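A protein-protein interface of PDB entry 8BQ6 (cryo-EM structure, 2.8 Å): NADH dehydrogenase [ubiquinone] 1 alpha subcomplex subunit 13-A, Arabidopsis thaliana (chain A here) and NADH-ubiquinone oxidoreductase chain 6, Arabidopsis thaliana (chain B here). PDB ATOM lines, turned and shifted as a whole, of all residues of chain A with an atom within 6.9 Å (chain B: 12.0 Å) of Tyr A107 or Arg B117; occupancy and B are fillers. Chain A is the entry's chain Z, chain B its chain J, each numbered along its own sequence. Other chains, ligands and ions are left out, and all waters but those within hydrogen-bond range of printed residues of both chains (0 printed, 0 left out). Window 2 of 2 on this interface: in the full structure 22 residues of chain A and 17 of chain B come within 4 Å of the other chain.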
ATOM      1  N   GLU A 100       9.963 -22.110  28.304  1.00  0.00           N
ATOM      2  CA  GLU A 100      10.318 -20.834  27.686  1.00  0.00           C
ATOM      3  C   GLU A 100      11.402 -21.006  26.628  1.00  0.00           C
ATOM      4  O   GLU A 100      11.364 -20.357  25.577  1.00  0.00           O
ATOM      5  CB  GLU A 100      10.778 -19.845  28.756  1.00  0.00           C
ATOM      6  CG  GLU A 100       9.692 -19.406  29.725  1.00  0.00           C
ATOM      7  CD  GLU A 100       8.721 -18.406  29.125  1.00  0.00           C
ATOM      8  OE1 GLU A 100       8.873 -18.046  27.938  1.00  0.00           O
ATOM      9  OE2 GLU A 100       7.799 -17.980  29.850  1.00  0.00           O
ATOM     10  N   TRP A 101      12.394 -21.854  26.902  1.00  0.00           N
ATOM     11  CA  TRP A 101      13.465 -22.093  25.946  1.00  0.00           C
ATOM     12  C   TRP A 101      12.947 -22.799  24.704  1.00  0.00           C
ATOM     13  O   TRP A 101      13.414 -22.534  23.592  1.00  0.00           O
ATOM     14  CB  TRP A 101      14.573 -22.910  26.602  1.00  0.00           C
ATOM     15  CG  TRP A 101      15.721 -23.167  25.698  1.00  0.00           C
ATOM     16  CD1 TRP A 101      16.098 -24.365  25.174  1.00  0.00           C
ATOM     17  CD2 TRP A 101      16.648 -22.201  25.201  1.00  0.00           C
ATOM     18  NE1 TRP A 101      17.207 -24.206  24.382  1.00  0.00           N
ATOM     19  CE2 TRP A 101      17.563 -22.884  24.383  1.00  0.00           C
ATOM     20  CE3 TRP A 101      16.796 -20.824  25.371  1.00  0.00           C
ATOM     21  CZ2 TRP A 101      18.608 -22.237  23.739  1.00  0.00           C
ATOM     22  CZ3 TRP A 101      17.829 -20.186  24.734  1.00  0.00           C
ATOM     23  CH2 TRP A 101      18.724 -20.889  23.928  1.00  0.00           C
ATOM     24  N   LYS A 102      11.987 -23.708  24.875  1.00  0.00           N
ATOM     25  CA  LYS A 102      11.325 -24.307  23.723  1.00  0.00           C
ATOM     26  C   LYS A 102      10.634 -23.241  22.880  1.00  0.00           C
ATOM     27  O   LYS A 102      10.787 -23.209  21.651  1.00  0.00           O
ATOM     28  CB  LYS A 102      10.328 -25.361  24.202  1.00  0.00           C
ATOM     29  CG  LYS A 102       9.853 -26.337  23.149  1.00  0.00           C
ATOM     30  CD  LYS A 102       9.398 -27.648  23.782  1.00  0.00           C
ATOM     31  CE  LYS A 102      10.263 -28.019  24.978  1.00  0.00           C
ATOM     32  NZ  LYS A 102      10.245 -29.478  25.275  1.00  0.00           N
ATOM     33  N   LYS A 103       9.891 -22.338  23.530  1.00  0.00           N
ATOM     34  CA  LYS A 103       9.223 -21.271  22.787  1.00  0.00           C
ATOM     35  C   LYS A 103      10.231 -20.401  22.038  1.00  0.00           C
ATOM     36  O   LYS A 103      10.034 -20.078  20.858  1.00  0.00           O
ATOM     37  CB  LYS A 103       8.383 -20.425  23.742  1.00  0.00           C
ATOM     38  CG  LYS A 103       6.908 -20.790  23.754  1.00  0.00           C
ATOM     39  CD  LYS A 103       6.245 -20.369  25.056  1.00  0.00           C
ATOM     40  CE  LYS A 103       6.450 -18.887  25.321  1.00  0.00           C
ATOM     41  NZ  LYS A 103       5.227 -18.095  25.026  1.00  0.00           N
ATOM     42  N   TYR A 104      11.325 -20.026  22.706  1.00  0.00           N
ATOM     43  CA  TYR A 104      12.340 -19.195  22.065  1.00  0.00           C
ATOM     44  C   TYR A 104      13.019 -19.932  20.919  1.00  0.00           C
ATOM     45  O   TYR A 104      13.432 -19.314  19.933  1.00  0.00           O
ATOM     46  CB  TYR A 104      13.377 -18.735  23.090  1.00  0.00           C
ATOM     47  CG  TYR A 104      14.600 -18.115  22.451  1.00  0.00           C
ATOM     48  CD1 TYR A 104      14.620 -16.774  22.107  1.00  0.00           C
ATOM     49  CD2 TYR A 104      15.726 -18.878  22.174  1.00  0.00           C
ATOM     50  CE1 TYR A 104      15.727 -16.207  21.514  1.00  0.00           C
ATOM     51  CE2 TYR A 104      16.833 -18.321  21.578  1.00  0.00           C
ATOM     52  CZ  TYR A 104      16.831 -16.985  21.251  1.00  0.00           C
ATOM     53  OH  TYR A 104      17.939 -16.427  20.658  1.00  0.00           O
ATOM     54  N   LEU A 105      13.170 -21.251  21.041  1.00  0.00           N
ATOM     55  CA  LEU A 105      13.780 -22.021  19.965  1.00  0.00           C
ATOM     56  C   LEU A 105      12.873 -22.062  18.742  1.00  0.00           C
ATOM     57  O   LEU A 105      13.350 -21.957  17.605  1.00  0.00           O
ATOM     58  CB  LEU A 105      14.100 -23.429  20.462  1.00  0.00           C
ATOM     59  CG  LEU A 105      15.531 -23.903  20.231  1.00  0.00           C
ATOM     60  CD1 LEU A 105      16.498 -22.771  20.514  1.00  0.00           C
ATOM     61  CD2 LEU A 105      15.830 -25.087  21.128  1.00  0.00           C
ATOM     62  N   GLU A 106      11.561 -22.199  18.954  1.00  0.00           N
ATOM     63  CA  GLU A 106      10.639 -22.096  17.825  1.00  0.00           C
ATOM     64  C   GLU A 106      10.705 -20.710  17.190  1.00  0.00           C
ATOM     65  O   GLU A 106      10.719 -20.583  15.958  1.00  0.00           O
ATOM     66  CB  GLU A 106       9.204 -22.431  18.247  1.00  0.00           C
ATOM     67  CG  GLU A 106       9.068 -23.559  19.255  1.00  0.00           C
ATOM     68  CD  GLU A 106       7.663 -23.683  19.824  1.00  0.00           C
ATOM     69  OE1 GLU A 106       7.058 -24.767  19.683  1.00  0.00           O
ATOM     70  OE2 GLU A 106       7.160 -22.696  20.403  1.00  0.00           O
ATOM     71  N   TYR A 107      10.769 -19.660  18.015  1.00  0.00           N
ATOM     72  CA  TYR A 107      10.899 -18.304  17.481  1.00  0.00           C
ATOM     73  C   TYR A 107      12.169 -18.146  16.649  1.00  0.00           C
ATOM     74  O   TYR A 107      12.147 -17.555  15.561  1.00  0.00           O
ATOM     75  CB  TYR A 107      10.884 -17.287  18.623  1.00  0.00           C
ATOM     76  CG  TYR A 107      11.515 -15.959  18.261  1.00  0.00           C
ATOM     77  CD1 TYR A 107      12.740 -15.585  18.797  1.00  0.00           C
ATOM     78  CD2 TYR A 107      10.897 -15.090  17.377  1.00  0.00           C
ATOM     79  CE1 TYR A 107      13.324 -14.377  18.468  1.00  0.00           C
ATOM     80  CE2 TYR A 107      11.473 -13.882  17.049  1.00  0.00           C
ATOM     81  CZ  TYR A 107      12.687 -13.532  17.593  1.00  0.00           C
ATOM     82  OH  TYR A 107      13.270 -12.331  17.264  1.00  0.00           O
ATOM     83  N   GLU A 108      13.293 -18.652  17.156  1.00  0.00           N
ATOM     84  CA  GLU A 108      14.555 -18.545  16.431  1.00  0.00           C
ATOM     85  C   GLU A 108      14.508 -19.315  15.119  1.00  0.00           C
ATOM     86  O   GLU A 108      14.990 -18.827  14.089  1.00  0.00           O
ATOM     87  CB  GLU A 108      15.699 -19.044  17.311  1.00  0.00           C
ATOM     88  CG  GLU A 108      17.003 -19.286  16.582  1.00  0.00           C
ATOM     89  CD  GLU A 108      18.155 -19.519  17.538  1.00  0.00           C
ATOM     90  OE1 GLU A 108      18.219 -18.820  18.571  1.00  0.00           O
ATOM     91  OE2 GLU A 108      18.998 -20.396  17.257  1.00  0.00           O
ATOM     92  N   ALA A 109      13.934 -20.521  15.135  1.00  0.00           N
ATOM     93  CA  ALA A 109      13.802 -21.284  13.900  1.00  0.00           C
ATOM     94  C   ALA A 109      12.951 -20.532  12.890  1.00  0.00           C
ATOM     95  O   ALA A 109      13.255 -20.522  11.692  1.00  0.00           O
ATOM     96  CB  ALA A 109      13.202 -22.659  14.190  1.00  0.00           C
ATOM     97  N   ASP A 110      11.882 -19.891  13.360  1.00  0.00           N
ATOM     98  CA  ASP A 110      11.026 -19.123  12.466  1.00  0.00           C
ATOM     99  C   ASP A 110      11.782 -17.955  11.844  1.00  0.00           C
ATOM    100  O   ASP A 110      11.835 -17.819  10.616  1.00  0.00           O
ATOM    101  CB  ASP A 110       9.811 -18.621  13.240  1.00  0.00           C
ATOM    102  CG  ASP A 110       8.591 -18.484  12.374  1.00  0.00           C
ATOM    103  OD1 ASP A 110       8.496 -17.480  11.639  1.00  0.00           O
ATOM    104  OD2 ASP A 110       7.721 -19.376  12.443  1.00  0.00           O
ATOM    105  N   VAL A 111      12.401 -17.119  12.681  1.00  0.00           N
ATOM    106  CA  VAL A 111      13.057 -15.915  12.179  1.00  0.00           C
ATOM    107  C   VAL A 111      14.244 -16.277  11.295  1.00  0.00           C
ATOM    108  O   VAL A 111      14.419 -15.719  10.206  1.00  0.00           O
ATOM    109  CB  VAL A 111      13.479 -15.009  13.352  1.00  0.00           C
ATOM    110  CG1 VAL A 111      14.588 -14.063  12.924  1.00  0.00           C
ATOM    111  CG2 VAL A 111      12.287 -14.235  13.882  1.00  0.00           C
ATOM    112  N   MET A 112      15.061 -17.230  11.737  1.00  0.00           N
ATOM    113  CA  MET A 112      16.279 -17.607  11.031  1.00  0.00           C
ATOM    114  C   MET A 112      16.030 -18.586   9.896  1.00  0.00           C
ATOM    115  O   MET A 112      16.992 -19.076   9.296  1.00  0.00           O
ATOM    116  CB  MET A 112      17.292 -18.201  12.006  1.00  0.00           C
ATOM    117  CG  MET A 112      17.804 -17.207  13.021  1.00  0.00           C
ATOM    118  SD  MET A 112      18.626 -15.811  12.242  1.00  0.00           S
ATOM    119  CE  MET A 112      20.057 -16.628  11.551  1.00  0.00           C
ATOM    120  N   LYS A 113      14.775 -18.899   9.603  1.00  0.00           N
ATOM    121  CA  LYS A 113      14.472 -19.668   8.408  1.00  0.00           C
ATOM    122  C   LYS A 113      14.906 -18.888   7.174  1.00  0.00           C
ATOM    123  O   LYS A 113      14.871 -17.655   7.161  1.00  0.00           O
ATOM    124  CB  LYS A 113      12.980 -19.976   8.351  1.00  0.00           C
ATOM    125  CG  LYS A 113      12.617 -21.103   7.421  1.00  0.00           C
ATOM    126  CD  LYS A 113      11.141 -21.403   7.531  1.00  0.00           C
ATOM    127  CE  LYS A 113      10.319 -20.211   7.074  1.00  0.00           C
ATOM    128  NZ  LYS A 113       9.333 -19.802   8.112  1.00  0.00           N
ATOM    129  N   LEU B 112      25.095  -6.729  23.787  1.00  0.00           N
ATOM    130  CA  LEU B 112      23.863  -7.406  23.409  1.00  0.00           C
ATOM    131  C   LEU B 112      22.815  -6.353  23.066  1.00  0.00           C
ATOM    132  O   LEU B 112      22.398  -5.580  23.933  1.00  0.00           O
ATOM    133  CB  LEU B 112      23.384  -8.302  24.543  1.00  0.00           C
ATOM    134  CG  LEU B 112      22.173  -9.157  24.215  1.00  0.00           C
ATOM    135  CD1 LEU B 112      22.561 -10.184  23.177  1.00  0.00           C
ATOM    136  CD2 LEU B 112      21.677  -9.818  25.480  1.00  0.00           C
ATOM    137  N   LEU B 113      22.392  -6.325  21.809  1.00  0.00           N
ATOM    138  CA  LEU B 113      21.417  -5.334  21.372  1.00  0.00           C
ATOM    139  C   LEU B 113      20.035  -5.675  21.922  1.00  0.00           C
ATOM    140  O   LEU B 113      19.636  -6.844  21.901  1.00  0.00           O
ATOM    141  CB  LEU B 113      21.373  -5.269  19.851  1.00  0.00           C
ATOM    142  CG  LEU B 113      22.648  -4.812  19.144  1.00  0.00           C
ATOM    143  CD1 LEU B 113      22.552  -5.143  17.674  1.00  0.00           C
ATOM    144  CD2 LEU B 113      22.889  -3.324  19.344  1.00  0.00           C
ATOM    145  N   PRO B 114      19.278  -4.691  22.410  1.00  0.00           N
ATOM    146  CA  PRO B 114      17.940  -4.969  22.957  1.00  0.00           C
ATOM    147  C   PRO B 114      16.925  -5.176  21.843  1.00  0.00           C
ATOM    148  O   PRO B 114      16.717  -4.301  20.999  1.00  0.00           O
ATOM    149  CB  PRO B 114      17.627  -3.715  23.779  1.00  0.00           C
ATOM    150  CG  PRO B 114      18.415  -2.638  23.131  1.00  0.00           C
ATOM    151  CD  PRO B 114      19.638  -3.267  22.513  1.00  0.00           C
ATOM    152  N   THR B 115      16.276  -6.332  21.858  1.00  0.00           N
ATOM    153  CA  THR B 115      15.311  -6.691  20.835  1.00  0.00           C
ATOM    154  C   THR B 115      13.892  -6.411  21.318  1.00  0.00           C
ATOM    155  O   THR B 115      13.646  -6.125  22.493  1.00  0.00           O
ATOM    156  CB  THR B 115      15.467  -8.164  20.451  1.00  0.00           C
ATOM    157  OG1 THR B 115      14.843  -8.989  21.442  1.00  0.00           O
ATOM    158  CG2 THR B 115      16.939  -8.521  20.375  1.00  0.00           C
ATOM    159  N   GLN B 116      12.951  -6.489  20.379  1.00  0.00           N
ATOM    160  CA  GLN B 116      11.540  -6.318  20.693  1.00  0.00           C
ATOM    161  C   GLN B 116      10.943  -7.668  21.067  1.00  0.00           C
ATOM    162  O   GLN B 116       9.908  -8.080  20.530  1.00  0.00           O
ATOM    163  CB  GLN B 116      10.801  -5.691  19.508  1.00  0.00           C
ATOM    164  CG  GLN B 116      11.448  -4.413  18.983  1.00  0.00           C
ATOM    165  CD  GLN B 116      11.037  -3.176  19.760  1.00  0.00           C
ATOM    166  OE1 GLN B 116       9.911  -3.082  20.246  1.00  0.00           O
ATOM    167  NE2 GLN B 116      11.945  -2.213  19.866  1.00  0.00           N
ATOM    168  N   ARG B 117      11.604  -8.358  21.990  1.00  0.00           N
ATOM    169  CA  ARG B 117      11.140  -9.625  22.526  1.00  0.00           C
ATOM    170  C   ARG B 117      11.527  -9.661  23.995  1.00  0.00           C
ATOM    171  O   ARG B 117      12.577  -9.140  24.380  1.00  0.00           O
ATOM    172  CB  ARG B 117      11.742 -10.811  21.759  1.00  0.00           C
ATOM    173  CG  ARG B 117      10.860 -12.044  21.723  1.00  0.00           C
ATOM    174  CD  ARG B 117      11.681 -13.319  21.821  1.00  0.00           C
ATOM    175  NE  ARG B 117      10.836 -14.507  21.852  1.00  0.00           N
ATOM    176  CZ  ARG B 117      10.486 -15.136  22.967  1.00  0.00           C
ATOM    177  NH1 ARG B 117      10.895 -14.716  24.152  1.00  0.00           N
ATOM    178  NH2 ARG B 117       9.703 -16.208  22.890  1.00  0.00           N
ATOM    179  N   ASN B 118      10.660 -10.245  24.818  1.00  0.00           N
ATOM    180  CA  ASN B 118      10.919 -10.311  26.256  1.00  0.00           C
ATOM    181  C   ASN B 118      11.959 -11.391  26.510  1.00  0.00           C
ATOM    182  O   ASN B 118      11.647 -12.584  26.531  1.00  0.00           O
ATOM    183  CB  ASN B 118       9.635 -10.578  27.037  1.00  0.00           C
ATOM    184  CG  ASN B 118       9.817 -10.377  28.536  1.00  0.00           C
ATOM    185  OD1 ASN B 118      10.629  -9.558  28.967  1.00  0.00           O
ATOM    186  ND2 ASN B 118       9.057 -11.119  29.334  1.00  0.00           N
ATOM    187  N   THR B 119      13.211 -10.970  26.694  1.00  0.00           N
ATOM    188  CA  THR B 119      14.275 -11.897  27.052  1.00  0.00           C
ATOM    189  C   THR B 119      14.371 -12.124  28.554  1.00  0.00           C
ATOM    190  O   THR B 119      15.172 -12.961  28.984  1.00  0.00           O
ATOM    191  CB  THR B 119      15.625 -11.394  26.527  1.00  0.00           C
ATOM    192  OG1 THR B 119      16.239 -10.545  27.504  1.00  0.00           O
ATOM    193  CG2 THR B 119      15.441 -10.616  25.231  1.00  0.00           C
ATOM    194  N   THR B 120      13.582 -11.405  29.359  1.00  0.00           N
ATOM    195  CA  THR B 120      13.607 -11.625  30.802  1.00  0.00           C
ATOM    196  C   THR B 120      13.067 -12.999  31.168  1.00  0.00           C
ATOM    197  O   THR B 120      13.407 -13.538  32.226  1.00  0.00           O
ATOM    198  CB  THR B 120      12.807 -10.539  31.524  1.00  0.00           C
ATOM    199  OG1 THR B 120      11.428 -10.626  31.146  1.00  0.00           O
ATOM    200  CG2 THR B 120      13.342  -9.159  31.181  1.00  0.00           C
ATOM    201  N   SER B 121      12.235 -13.585  30.306  1.00  0.00           N
ATOM    202  CA  SER B 121      11.687 -14.904  30.587  1.00  0.00           C
ATOM    203  C   SER B 121      12.729 -16.008  30.467  1.00  0.00           C
ATOM    204  O   SER B 121      12.452 -17.146  30.858  1.00  0.00           O
ATOM    205  CB  SER B 121      10.514 -15.186  29.651  1.00  0.00           C
ATOM    206  OG  SER B 121      10.950 -15.856  28.483  1.00  0.00           O
ATOM    207  N   LEU B 122      13.909 -15.709  29.931  1.00  0.00           N
ATOM    208  CA  LEU B 122      14.967 -16.703  29.818  1.00  0.00           C
ATOM    209  C   LEU B 122      16.012 -16.583  30.913  1.00  0.00           C
ATOM    210  O   LEU B 122      17.011 -17.309  30.880  1.00  0.00           O
ATOM    211  CB  LEU B 122      15.644 -16.610  28.454  1.00  0.00           C
ATOM    212  CG  LEU B 122      14.890 -17.417  27.402  1.00  0.00           C
ATOM    213  CD1 LEU B 122      15.262 -16.953  26.013  1.00  0.00           C
ATOM    214  CD2 LEU B 122      15.127 -18.907  27.582  1.00  0.00           C
ATOM    215  N   ARG B 123      15.820 -15.678  31.862  1.00  0.00           N
ATOM    216  CA  ARG B 123      16.658 -15.653  33.049  1.00  0.00           C
ATOM    217  C   ARG B 123      16.430 -16.929  33.848  1.00  0.00           C
ATOM    218  O   ARG B 123      15.314 -17.193  34.305  1.00  0.00           O
ATOM    219  CB  ARG B 123      16.339 -14.419  33.888  1.00  0.00           C
ATOM    220  CG  ARG B 123      17.565 -13.705  34.414  1.00  0.00           C
ATOM    221  CD  ARG B 123      17.372 -12.197  34.474  1.00  0.00           C
ATOM    222  NE  ARG B 123      17.432 -11.561  33.164  1.00  0.00           N
ATOM    223  CZ  ARG B 123      17.162 -10.281  32.943  1.00  0.00           C
ATOM    224  NH1 ARG B 123      16.790  -9.475  33.925  1.00  0.00           N
ATOM    225  NH2 ARG B 123      17.276  -9.795  31.710  1.00  0.00           N
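The side-chain carboxylate of Glu A100 is in hydrogen-bond range of the side-chain hydroxyl of Ser B121 (3.1 Å).
Of the printed residues of chain B, Glu A100 touches Ser B121 (3.1 Å).
Of the printed residues of chain B, Trp A101 touches Leu B122.
No residue of chain B comes within 4 Å of Glu A106.
Of chain B, only Arg B117 comes within 4 Å of Tyr A107.
No residue of chain B comes within 4 Å of Glu A108.
No residue of chain B comes within 4 Å of Ala A109.
No residue of chain B comes within 4 Å of Val A111.
Arg B117 touches one residue of chain A.
Asn B118 touches none of the printed residues of chain A.
Of the printed residues of chain A, Ser B121 touches Glu A100.
The nearest residue of chain B that does not touch Tyr A107 is Thr B115 (5.6 Å).
The nearest residue of chain A that does not touch Arg B117 is Tyr A104 (4.1 Å).
The nearest printed residue of chain A that does not touch Ser B121 is Trp A101 (6.1 Å).
The side-chain hydroxyl of Thr B115 lies close to the backbone NH of Arg B117.
The side-chain carboxylate (OE1) of Glu A108 sits at hydrogen-bond distance from the side-chain hydroxyl (OH) of Tyr A104, 3.2 Å away.
Leu B122 touches Trp A101.
Leu B122 touches Tyr A104.
Tyr A107 touches Arg B117.
Of the 14 printed residues of chain A, 4 touch a printed residue of chain B.
Printed residues of chain A that touch a printed residue of chain B: Glu A100, Trp A101, Tyr A104 and Tyr A107.
Hydrophobic or aromatic side chains of chain A that line the printed part of chain B: Trp A101, Tyr A104 and Tyr A107.
Among the printed residues, 4 pairs touch across the chains.
Among the printed residues, no Asp or Glu carboxylate lies within 4 Å of a Lys or Arg side-chain nitrogen of the other chain.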
